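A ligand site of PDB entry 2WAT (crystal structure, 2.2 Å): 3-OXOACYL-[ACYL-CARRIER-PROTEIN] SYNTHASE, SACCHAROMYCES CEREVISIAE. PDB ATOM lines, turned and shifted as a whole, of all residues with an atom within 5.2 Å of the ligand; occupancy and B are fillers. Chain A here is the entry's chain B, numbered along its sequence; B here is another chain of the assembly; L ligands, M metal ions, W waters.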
ATOM      1  N   TYR A  33       2.780 -21.329 -14.542  1.00  0.00           N
ATOM      2  CA  TYR A  33       3.989 -21.369 -15.342  1.00  0.00           C
ATOM      3  C   TYR A  33       4.737 -22.683 -15.145  1.00  0.00           C
ATOM      4  O   TYR A  33       5.034 -23.403 -16.101  1.00  0.00           O
ATOM      5  CB  TYR A  33       4.916 -20.187 -15.016  1.00  0.00           C
ATOM      6  CG  TYR A  33       6.193 -20.241 -15.794  1.00  0.00           C
ATOM      7  CD1 TYR A  33       6.294 -19.645 -17.057  1.00  0.00           C
ATOM      8  CD2 TYR A  33       7.305 -20.909 -15.304  1.00  0.00           C
ATOM      9  CE1 TYR A  33       7.458 -19.706 -17.785  1.00  0.00           C
ATOM     10  CE2 TYR A  33       8.477 -20.981 -16.027  1.00  0.00           C
ATOM     11  CZ  TYR A  33       8.550 -20.370 -17.272  1.00  0.00           C
ATOM     12  OH  TYR A  33       9.714 -20.431 -18.000  1.00  0.00           O
ATOM     13  N   GLN A  37       5.805 -26.293 -17.836  1.00  0.00           N
ATOM     14  CA  GLN A  37       7.150 -26.530 -18.349  1.00  0.00           C
ATOM     15  C   GLN A  37       7.418 -28.009 -18.621  1.00  0.00           C
ATOM     16  O   GLN A  37       6.713 -28.861 -18.115  1.00  0.00           O
ATOM     17  CB  GLN A  37       8.186 -25.981 -17.375  1.00  0.00           C
ATOM     18  CG  GLN A  37       8.052 -24.495 -17.122  1.00  0.00           C
ATOM     19  CD  GLN A  37       7.803 -23.716 -18.392  1.00  0.00           C
ATOM     20  OE1 GLN A  37       6.775 -23.055 -18.539  1.00  0.00           O
ATOM     21  NE2 GLN A  37       8.735 -23.796 -19.330  1.00  0.00           N
ATOM     22  N   SER A  43      11.177 -27.040 -12.622  1.00  0.00           N
ATOM     23  CA  SER A  43      10.765 -25.639 -12.744  1.00  0.00           C
ATOM     24  C   SER A  43      10.369 -25.074 -11.382  1.00  0.00           C
ATOM     25  O   SER A  43      10.787 -23.981 -11.029  1.00  0.00           O
ATOM     26  CB  SER A  43       9.608 -25.501 -13.726  1.00  0.00           C
ATOM     27  OG  SER A  43       9.476 -24.160 -14.156  1.00  0.00           O
ATOM     28  N   THR A  47      12.190 -22.019  -9.317  1.00  0.00           N
ATOM     29  CA  THR A  47      11.433 -20.886  -8.800  1.00  0.00           C
ATOM     30  C   THR A  47      11.591 -20.754  -7.283  1.00  0.00           C
ATOM     31  O   THR A  47      11.705 -19.658  -6.760  1.00  0.00           O
ATOM     32  CB  THR A  47       9.934 -20.998  -9.174  1.00  0.00           C
ATOM     33  OG1 THR A  47       9.798 -20.982 -10.599  1.00  0.00           O
ATOM     34  CG2 THR A  47       9.143 -19.834  -8.611  1.00  0.00           C
ATOM     35  N   ARG A  76       7.328 -13.514 -15.291  1.00  0.00           N
ATOM     36  CA  ARG A  76       8.129 -13.672 -16.490  1.00  0.00           C
ATOM     37  C   ARG A  76       8.124 -12.430 -17.381  1.00  0.00           C
ATOM     38  O   ARG A  76       7.132 -11.702 -17.453  1.00  0.00           O
ATOM     39  CB  ARG A  76       7.703 -14.930 -17.221  1.00  0.00           C
ATOM     40  CG  ARG A  76       7.168 -16.017 -16.311  1.00  0.00           C
ATOM     41  CD  ARG A  76       8.099 -16.370 -15.147  1.00  0.00           C
ATOM     42  NE  ARG A  76       9.280 -17.092 -15.597  1.00  0.00           N
ATOM     43  CZ  ARG A  76       9.891 -18.063 -14.916  1.00  0.00           C
ATOM     44  NH1 ARG A  76       9.443 -18.460 -13.736  1.00  0.00           N
ATOM     45  NH2 ARG A  76      10.962 -18.627 -15.433  1.00  0.00           N
ATOM     46  N   ASN A  80       9.585 -16.370 -20.864  1.00  0.00           N
ATOM     47  CA  ASN A  80      10.233 -17.322 -19.960  1.00  0.00           C
ATOM     48  C   ASN A  80      11.297 -16.787 -19.004  1.00  0.00           C
ATOM     49  O   ASN A  80      11.712 -17.489 -18.087  1.00  0.00           O
ATOM     50  CB  ASN A  80      10.815 -18.496 -20.752  1.00  0.00           C
ATOM     51  CG  ASN A  80       9.773 -19.274 -21.530  1.00  0.00           C
ATOM     52  OD1 ASN A  80       9.188 -20.238 -21.014  1.00  0.00           O
ATOM     53  ND2 ASN A  80       9.554 -18.889 -22.771  1.00  0.00           N
ATOM     54  N   ALA A  81      11.757 -15.558 -19.222  1.00  0.00           N
ATOM     55  CA  ALA A  81      12.784 -14.954 -18.365  1.00  0.00           C
ATOM     56  C   ALA A  81      12.200 -14.501 -17.026  1.00  0.00           C
ATOM     57  O   ALA A  81      11.135 -13.879 -17.001  1.00  0.00           O
ATOM     58  CB  ALA A  81      13.491 -13.786 -19.100  1.00  0.00           C
ATOM     59  N   PRO A  82      12.872 -14.818 -15.917  1.00  0.00           N
ATOM     60  CA  PRO A  82      12.324 -14.483 -14.590  1.00  0.00           C
ATOM     61  C   PRO A  82      12.555 -13.019 -14.155  1.00  0.00           C
ATOM     62  O   PRO A  82      13.671 -12.520 -14.282  1.00  0.00           O
ATOM     63  CB  PRO A  82      13.063 -15.443 -13.647  1.00  0.00           C
ATOM     64  CG  PRO A  82      14.355 -15.773 -14.355  1.00  0.00           C
ATOM     65  CD  PRO A  82      14.126 -15.611 -15.843  1.00  0.00           C
ATOM     66  N   SER A 105      18.128 -14.695 -11.708  1.00  0.00           N
ATOM     67  CA  SER A 105      18.345 -15.646 -12.783  1.00  0.00           C
ATOM     68  C   SER A 105      18.255 -17.076 -12.237  1.00  0.00           C
ATOM     69  O   SER A 105      18.584 -17.325 -11.089  1.00  0.00           O
ATOM     70  CB  SER A 105      19.704 -15.414 -13.447  1.00  0.00           C
ATOM     71  OG  SER A 105      19.880 -16.316 -14.532  1.00  0.00           O
ATOM     72  N   ILE A 106      17.797 -17.991 -13.071  1.00  0.00           N
ATOM     73  CA  ILE A 106      17.592 -19.376 -12.658  1.00  0.00           C
ATOM     74  C   ILE A 106      18.265 -20.348 -13.620  1.00  0.00           C
ATOM     75  O   ILE A 106      18.370 -20.076 -14.820  1.00  0.00           O
ATOM     76  CB  ILE A 106      16.101 -19.715 -12.613  1.00  0.00           C
ATOM     77  CG1 ILE A 106      15.370 -18.825 -11.591  1.00  0.00           C
ATOM     78  CG2 ILE A 106      15.878 -21.180 -12.292  1.00  0.00           C
ATOM     79  CD1 ILE A 106      13.851 -18.897 -11.724  1.00  0.00           C
ATOM     80  N   SER A 107      18.740 -21.476 -13.091  1.00  0.00           N
ATOM     81  CA  SER A 107      19.316 -22.526 -13.911  1.00  0.00           C
ATOM     82  C   SER A 107      19.116 -23.860 -13.186  1.00  0.00           C
ATOM     83  O   SER A 107      18.980 -23.892 -11.980  1.00  0.00           O
ATOM     84  CB  SER A 107      20.816 -22.283 -14.134  1.00  0.00           C
ATOM     85  OG  SER A 107      21.388 -23.309 -14.932  1.00  0.00           O
ATOM     86  N   HIS A 108      19.100 -24.962 -13.921  1.00  0.00           N
ATOM     87  CA  HIS A 108      19.084 -26.287 -13.279  1.00  0.00           C
ATOM     88  C   HIS A 108      19.877 -27.335 -14.035  1.00  0.00           C
ATOM     89  O   HIS A 108      20.113 -27.215 -15.230  1.00  0.00           O
ATOM     90  CB  HIS A 108      17.649 -26.808 -13.012  1.00  0.00           C
ATOM     91  CG  HIS A 108      16.561 -26.019 -13.657  1.00  0.00           C
ATOM     92  ND1 HIS A 108      16.216 -26.177 -14.991  1.00  0.00           N
ATOM     93  CD2 HIS A 108      15.722 -25.080 -13.166  1.00  0.00           C
ATOM     94  CE1 HIS A 108      15.220 -25.355 -15.279  1.00  0.00           C
ATOM     95  NE2 HIS A 108      14.906 -24.675 -14.189  1.00  0.00           N
ATOM     96  N   VAL B   6      22.755 -16.741 -14.443  1.00  0.00           N
ATOM     97  CA  VAL B   6      23.429 -17.895 -13.845  1.00  0.00           C
ATOM     98  C   VAL B   6      23.190 -19.127 -14.713  1.00  0.00           C
ATOM     99  O   VAL B   6      22.124 -19.302 -15.299  1.00  0.00           O
ATOM    100  CB  VAL B   6      22.946 -18.184 -12.411  1.00  0.00           C
ATOM    101  CG1 VAL B   6      21.483 -18.625 -12.396  1.00  0.00           C
ATOM    102  CG2 VAL B   6      23.811 -19.254 -11.755  1.00  0.00           C
ATOM    103  N   ASP B   7      24.207 -19.973 -14.810  1.00  0.00           N
ATOM    104  CA  ASP B   7      24.049 -21.215 -15.536  1.00  0.00           C
ATOM    105  C   ASP B   7      24.870 -22.303 -14.887  1.00  0.00           C
ATOM    106  O   ASP B   7      26.013 -22.093 -14.487  1.00  0.00           O
ATOM    107  CB  ASP B   7      24.439 -21.076 -17.006  1.00  0.00           C
ATOM    108  CG  ASP B   7      23.984 -22.271 -17.845  1.00  0.00           C
ATOM    109  OD1 ASP B   7      22.759 -22.451 -18.025  1.00  0.00           O
ATOM    110  OD2 ASP B   7      24.842 -23.023 -18.343  1.00  0.00           O
ATOM    111  N   VAL B   8      24.275 -23.488 -14.789  1.00  0.00           N
ATOM    112  CA  VAL B   8      24.961 -24.628 -14.223  1.00  0.00           C
ATOM    113  C   VAL B   8      24.961 -25.739 -15.271  1.00  0.00           C
ATOM    114  O   VAL B   8      23.956 -25.960 -15.942  1.00  0.00           O
ATOM    115  CB  VAL B   8      24.309 -25.084 -12.909  1.00  0.00           C
ATOM    116  CG1 VAL B   8      22.944 -25.725 -13.166  1.00  0.00           C
ATOM    117  CG2 VAL B   8      25.213 -26.023 -12.166  1.00  0.00           C
ATOM    118  N   GLU B  52      26.279 -19.083 -21.376  1.00  0.00           N
ATOM    119  CA  GLU B  52      24.852 -19.130 -21.059  1.00  0.00           C
ATOM    120  C   GLU B  52      24.488 -18.102 -20.004  1.00  0.00           C
ATOM    121  O   GLU B  52      23.473 -17.433 -20.111  1.00  0.00           O
ATOM    122  CB  GLU B  52      24.444 -20.516 -20.575  1.00  0.00           C
ATOM    123  CG  GLU B  52      24.620 -21.614 -21.595  1.00  0.00           C
ATOM    124  CD  GLU B  52      23.508 -21.645 -22.620  1.00  0.00           C
ATOM    125  OE1 GLU B  52      22.912 -20.579 -22.878  1.00  0.00           O
ATOM    126  OE2 GLU B  52      23.232 -22.731 -23.163  1.00  0.00           O
ATOM    127  N   PHE B  55      24.440 -14.701 -21.548  1.00  0.00           N
ATOM    128  CA  PHE B  55      23.242 -14.519 -22.356  1.00  0.00           C
ATOM    129  C   PHE B  55      22.026 -14.179 -21.493  1.00  0.00           C
ATOM    130  O   PHE B  55      21.251 -13.277 -21.827  1.00  0.00           O
ATOM    131  CB  PHE B  55      22.929 -15.766 -23.196  1.00  0.00           C
ATOM    132  CG  PHE B  55      21.549 -15.734 -23.794  1.00  0.00           C
ATOM    133  CD1 PHE B  55      21.318 -15.067 -24.985  1.00  0.00           C
ATOM    134  CD2 PHE B  55      20.490 -16.336 -23.147  1.00  0.00           C
ATOM    135  CE1 PHE B  55      20.055 -15.017 -25.527  1.00  0.00           C
ATOM    136  CE2 PHE B  55      19.206 -16.286 -23.697  1.00  0.00           C
ATOM    137  CZ  PHE B  55      19.004 -15.626 -24.889  1.00  0.00           C
ATOM    138  N   LYS B  56      21.846 -14.903 -20.393  1.00  0.00           N
ATOM    139  CA  LYS B  56      20.696 -14.686 -19.520  1.00  0.00           C
ATOM    140  C   LYS B  56      20.707 -13.306 -18.893  1.00  0.00           C
ATOM    141  O   LYS B  56      19.659 -12.773 -18.532  1.00  0.00           O
ATOM    142  CB  LYS B  56      20.641 -15.733 -18.417  1.00  0.00           C
ATOM    143  CG  LYS B  56      20.280 -17.133 -18.891  1.00  0.00           C
ATOM    144  CD  LYS B  56      20.263 -18.105 -17.718  1.00  0.00           C
ATOM    145  CE  LYS B  56      20.070 -19.530 -18.177  1.00  0.00           C
ATOM    146  NZ  LYS B  56      20.158 -20.442 -17.024  1.00  0.00           N
ATOM    147  N   VAL B  60      17.418 -10.385 -23.204  1.00  0.00           N
ATOM    148  CA  VAL B  60      16.946 -10.416 -24.588  1.00  0.00           C
ATOM    149  C   VAL B  60      16.185 -11.740 -24.771  1.00  0.00           C
ATOM    150  O   VAL B  60      16.386 -12.673 -24.004  1.00  0.00           O
ATOM    151  CB  VAL B  60      18.122 -10.260 -25.574  1.00  0.00           C
ATOM    152  CG1 VAL B  60      18.869  -8.959 -25.309  1.00  0.00           C
ATOM    153  CG2 VAL B  60      19.058 -11.452 -25.462  1.00  0.00           C
ATOM    154  N   LYS B  61      15.235 -11.831 -25.695  1.00  0.00           N
ATOM    155  CA  LYS B  61      14.479 -13.087 -25.790  1.00  0.00           C
ATOM    156  C   LYS B  61      15.275 -14.168 -26.519  1.00  0.00           C
ATOM    157  O   LYS B  61      15.118 -15.368 -26.262  1.00  0.00           O
ATOM    158  CB  LYS B  61      13.115 -12.880 -26.444  1.00  0.00           C
ATOM    159  CG  LYS B  61      12.233 -14.115 -26.376  1.00  0.00           C
ATOM    160  CD  LYS B  61      10.772 -13.801 -26.713  1.00  0.00           C
ATOM    161  CE  LYS B  61      10.625 -13.256 -28.123  1.00  0.00           C
ATOM    162  NZ  LYS B  61       9.259 -12.690 -28.362  1.00  0.00           N
HETATM  163  N1  LIG L   1      16.706 -14.794 -20.560  1.00  0.00           N
HETATM  164  C1  LIG L   1      17.134 -15.016 -19.279  1.00  0.00           C
HETATM  165  N2  LIG L   1      16.741 -16.146 -18.589  1.00  0.00           N
HETATM  166  C2  LIG L   1      15.920 -17.050 -19.194  1.00  0.00           C
HETATM  167  C3  LIG L   1      15.469 -16.841 -20.488  1.00  0.00           C
HETATM  168  C4  LIG L   1      15.863 -15.703 -21.182  1.00  0.00           C
HETATM  169  N3  LIG L   1      15.557 -15.579 -22.472  1.00  0.00           N
HETATM  170  N4  LIG L   1      14.685 -17.875 -20.828  1.00  0.00           N
HETATM  171  C5  LIG L   1      14.617 -18.743 -19.780  1.00  0.00           C
HETATM  172  N5  LIG L   1      15.379 -18.240 -18.761  1.00  0.00           N
HETATM  173  C6  LIG L   1      15.631 -18.909 -17.480  1.00  0.00           C
HETATM  174  C7  LIG L   1      14.335 -19.557 -17.031  1.00  0.00           C
HETATM  175  O1  LIG L   1      14.184 -19.281 -15.664  1.00  0.00           O
HETATM  176  C8  LIG L   1      14.540 -21.047 -17.199  1.00  0.00           C
HETATM  177  O2  LIG L   1      14.022 -21.773 -16.125  1.00  0.00           O
HETATM  178  P1  LIG L   1      12.423 -21.854 -15.939  1.00  0.00           P
HETATM  179  O3  LIG L   1      12.121 -20.826 -14.881  1.00  0.00           O
HETATM  180  O4  LIG L   1      12.005 -23.235 -15.491  1.00  0.00           O
HETATM  181  O5  LIG L   1      11.736 -21.551 -17.230  1.00  0.00           O
HETATM  182  C9  LIG L   1      16.055 -21.183 -17.220  1.00  0.00           C
HETATM  183  O6  LIG L   1      16.565 -19.946 -17.684  1.00  0.00           O
HETATM  184  C10 LIG L   1      16.525 -22.349 -18.082  1.00  0.00           C
HETATM  185  O7  LIG L   1      17.918 -22.345 -17.888  1.00  0.00           O
HETATM  186  P2  LIG L   1      18.739 -23.702 -17.678  1.00  0.00           P
HETATM  187  O8  LIG L   1      17.946 -24.607 -16.763  1.00  0.00           O
HETATM  188  O9  LIG L   1      20.069 -23.340 -17.050  1.00  0.00           O
HETATM  189  O10 LIG L   1      19.000 -24.473 -19.066  1.00  0.00           O
HETATM  190  P3  LIG L   1      18.034 -24.622 -20.342  1.00  0.00           P
HETATM  191  O11 LIG L   1      18.743 -25.520 -21.323  1.00  0.00           O
HETATM  192  O12 LIG L   1      16.695 -25.225 -19.955  1.00  0.00           O
HETATM  193  O13 LIG L   1      17.847 -23.140 -20.961  1.00  0.00           O
HETATM  194  C11 LIG L   1      18.587 -21.161 -22.192  1.00  0.00           C
HETATM  195  C12 LIG L   1      18.928 -22.265 -21.174  1.00  0.00           C
HETATM  196  C13 LIG L   1      17.496 -20.254 -21.643  1.00  0.00           C
HETATM  197  C14 LIG L   1      19.851 -20.338 -22.388  1.00  0.00           C
HETATM  198  C15 LIG L   1      18.159 -21.708 -23.555  1.00  0.00           C
HETATM  199  O14 LIG L   1      19.202 -22.450 -24.136  1.00  0.00           O
HETATM  200  C16 LIG L   1      16.887 -22.510 -23.537  1.00  0.00           C
HETATM  201  O15 LIG L   1      15.710 -22.014 -22.950  1.00  0.00           O
HETATM  202  N6  LIG L   1      16.958 -23.692 -24.129  1.00  0.00           N
HETATM  203  C17 LIG L   1      16.200 -24.846 -23.689  1.00  0.00           C
HETATM  204  C18 LIG L   1      15.034 -25.139 -24.620  1.00  0.00           C
HETATM  205  C19 LIG L   1      15.546 -25.591 -25.962  1.00  0.00           C
HETATM  206  O16 LIG L   1      16.745 -25.905 -26.114  1.00  0.00           O
HETATM  207  N7  LIG L   1      14.638 -25.628 -26.941  1.00  0.00           N
HETATM  208  C20 LIG L   1      14.992 -25.910 -28.307  1.00  0.00           C
HETATM  209  C21 LIG L   1      13.985 -26.821 -28.976  1.00  0.00           C
HETATM  210  S1  LIG L   1      14.765 -28.109 -29.948  1.00  0.00           S
HETATM  211 MG    MG M   1      21.652 -26.132 -17.600  1.00  0.00          MG
HETATM  212  O   HOH W   1      18.383 -12.878 -21.700  1.00  0.00           O
HETATM  213  O   HOH W   2      14.546 -23.152 -20.800  1.00  0.00           O
HETATM  214  O   HOH W   3      11.469 -21.670 -12.568  1.00  0.00           O
HETATM  215  O   HOH W   4      11.657 -24.712 -17.790  1.00  0.00           O
HETATM  216  O   HOH W   5      21.807 -22.626 -26.319  1.00  0.00           O
HETATM  217  O   HOH W   6      17.628 -15.718 -15.979  1.00  0.00           O
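An oxygen (O4) of the ligand sits at hydrogen-bond distance from the side-chain hydroxyl (OG) of Ser 43, 3.0 Å away.
The backbone carbonyl oxygen of Val 60 of chain B sits at hydrogen-bond distance from a nitrogen (N3) of the ligand, 3.4 Å away.
An oxygen (O9) of the ligand lies within salt-bridge range of the side-chain amino group (NZ) of Lys 56 of chain B (2.9 Å).
OG of Ser 107 sits at hydrogen-bond distance from O9 of the ligand (2.5 Å).
An oxygen (O3) of the ligand lies within salt-bridge range of the guanidinium group of Arg 76, 2.5 Å away.
An oxygen (O8) of the ligand is in hydrogen-bond range of the backbone NH (N) of His 108, 3.1 Å away.
OH of Tyr 33 lies within hydrogen-bond range of O5 of the ligand (2.4 Å).
An oxygen (O8) of the ligand is in hydrogen-bond range of a ring nitrogen (ND1) of His 108 (2.9 Å).
The side-chain carboxylate of Asp 7 of chain B sits close to an oxygen (O9) of the ligand (3.0 Å).
OG1 of Thr 47 sits at hydrogen-bond distance from O of Ser 43 (3.2 Å).
The side-chain hydroxyl (OG) of Ser 107 lies close to the side-chain carboxylate (OD1) of Asp 7 of chain B (3.5 Å).
The side-chain amino group of Lys 56 of chain B is in salt-bridge range of the side-chain carboxylate of Asp 7 of chain B.
The side-chain hydroxyl of Tyr 33 sits at hydrogen-bond distance from the guanidinium group of Arg 76, at 3.4 Å.
The guanidinium group (NH2) of Arg 76 is in hydrogen-bond range of the backbone carbonyl oxygen (O) of Asn 80 (3.0 Å).
OG of Ser 107 lies within hydrogen-bond range of N of Val 8 of chain B, 2.9 Å away.
OH of Tyr 33 lies within hydrogen-bond range of OD1 of Asn 80 (3.1 Å).
O of Ile 106 lies within hydrogen-bond range of NZ of Lys 56 of chain B (2.9 Å).
O of Ile 106 lies close to O6 of the ligand (3.4 Å).
O of Asn 80 touches C7 of the ligand, 3.5 Å away.
Ala 81 touches the ligand.
Pro 82 touches the ligand.
Glu 52 of chain B touches the ligand (OE1 to C14, 3.1 Å).
Phe 55 of chain B touches the ligand.
Lys 61 of chain B touches the ligand.
Of the 20 residues printed, 15 come within 4 Å of the ligand.
Water W3 lies within hydrogen-bond range of O3 of the ligand (2.5 Å), OG1 of Thr 47 (2.7 Å) and O of Ser 43 (2.9 Å).
Water W4 bridges O4 of the ligand (2.8 Å) and NE2 of Gln 37 (3.4 Å).
Water W6 lies within hydrogen-bond range of OG of Ser 105 (2.7 Å) and N2 of the ligand (2.8 Å).
Water W5 bridges an oxygen (O14) of the ligand (3.4 Å) and the side-chain carboxylate (OE2) of Glu 52 of chain B (3.5 Å).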
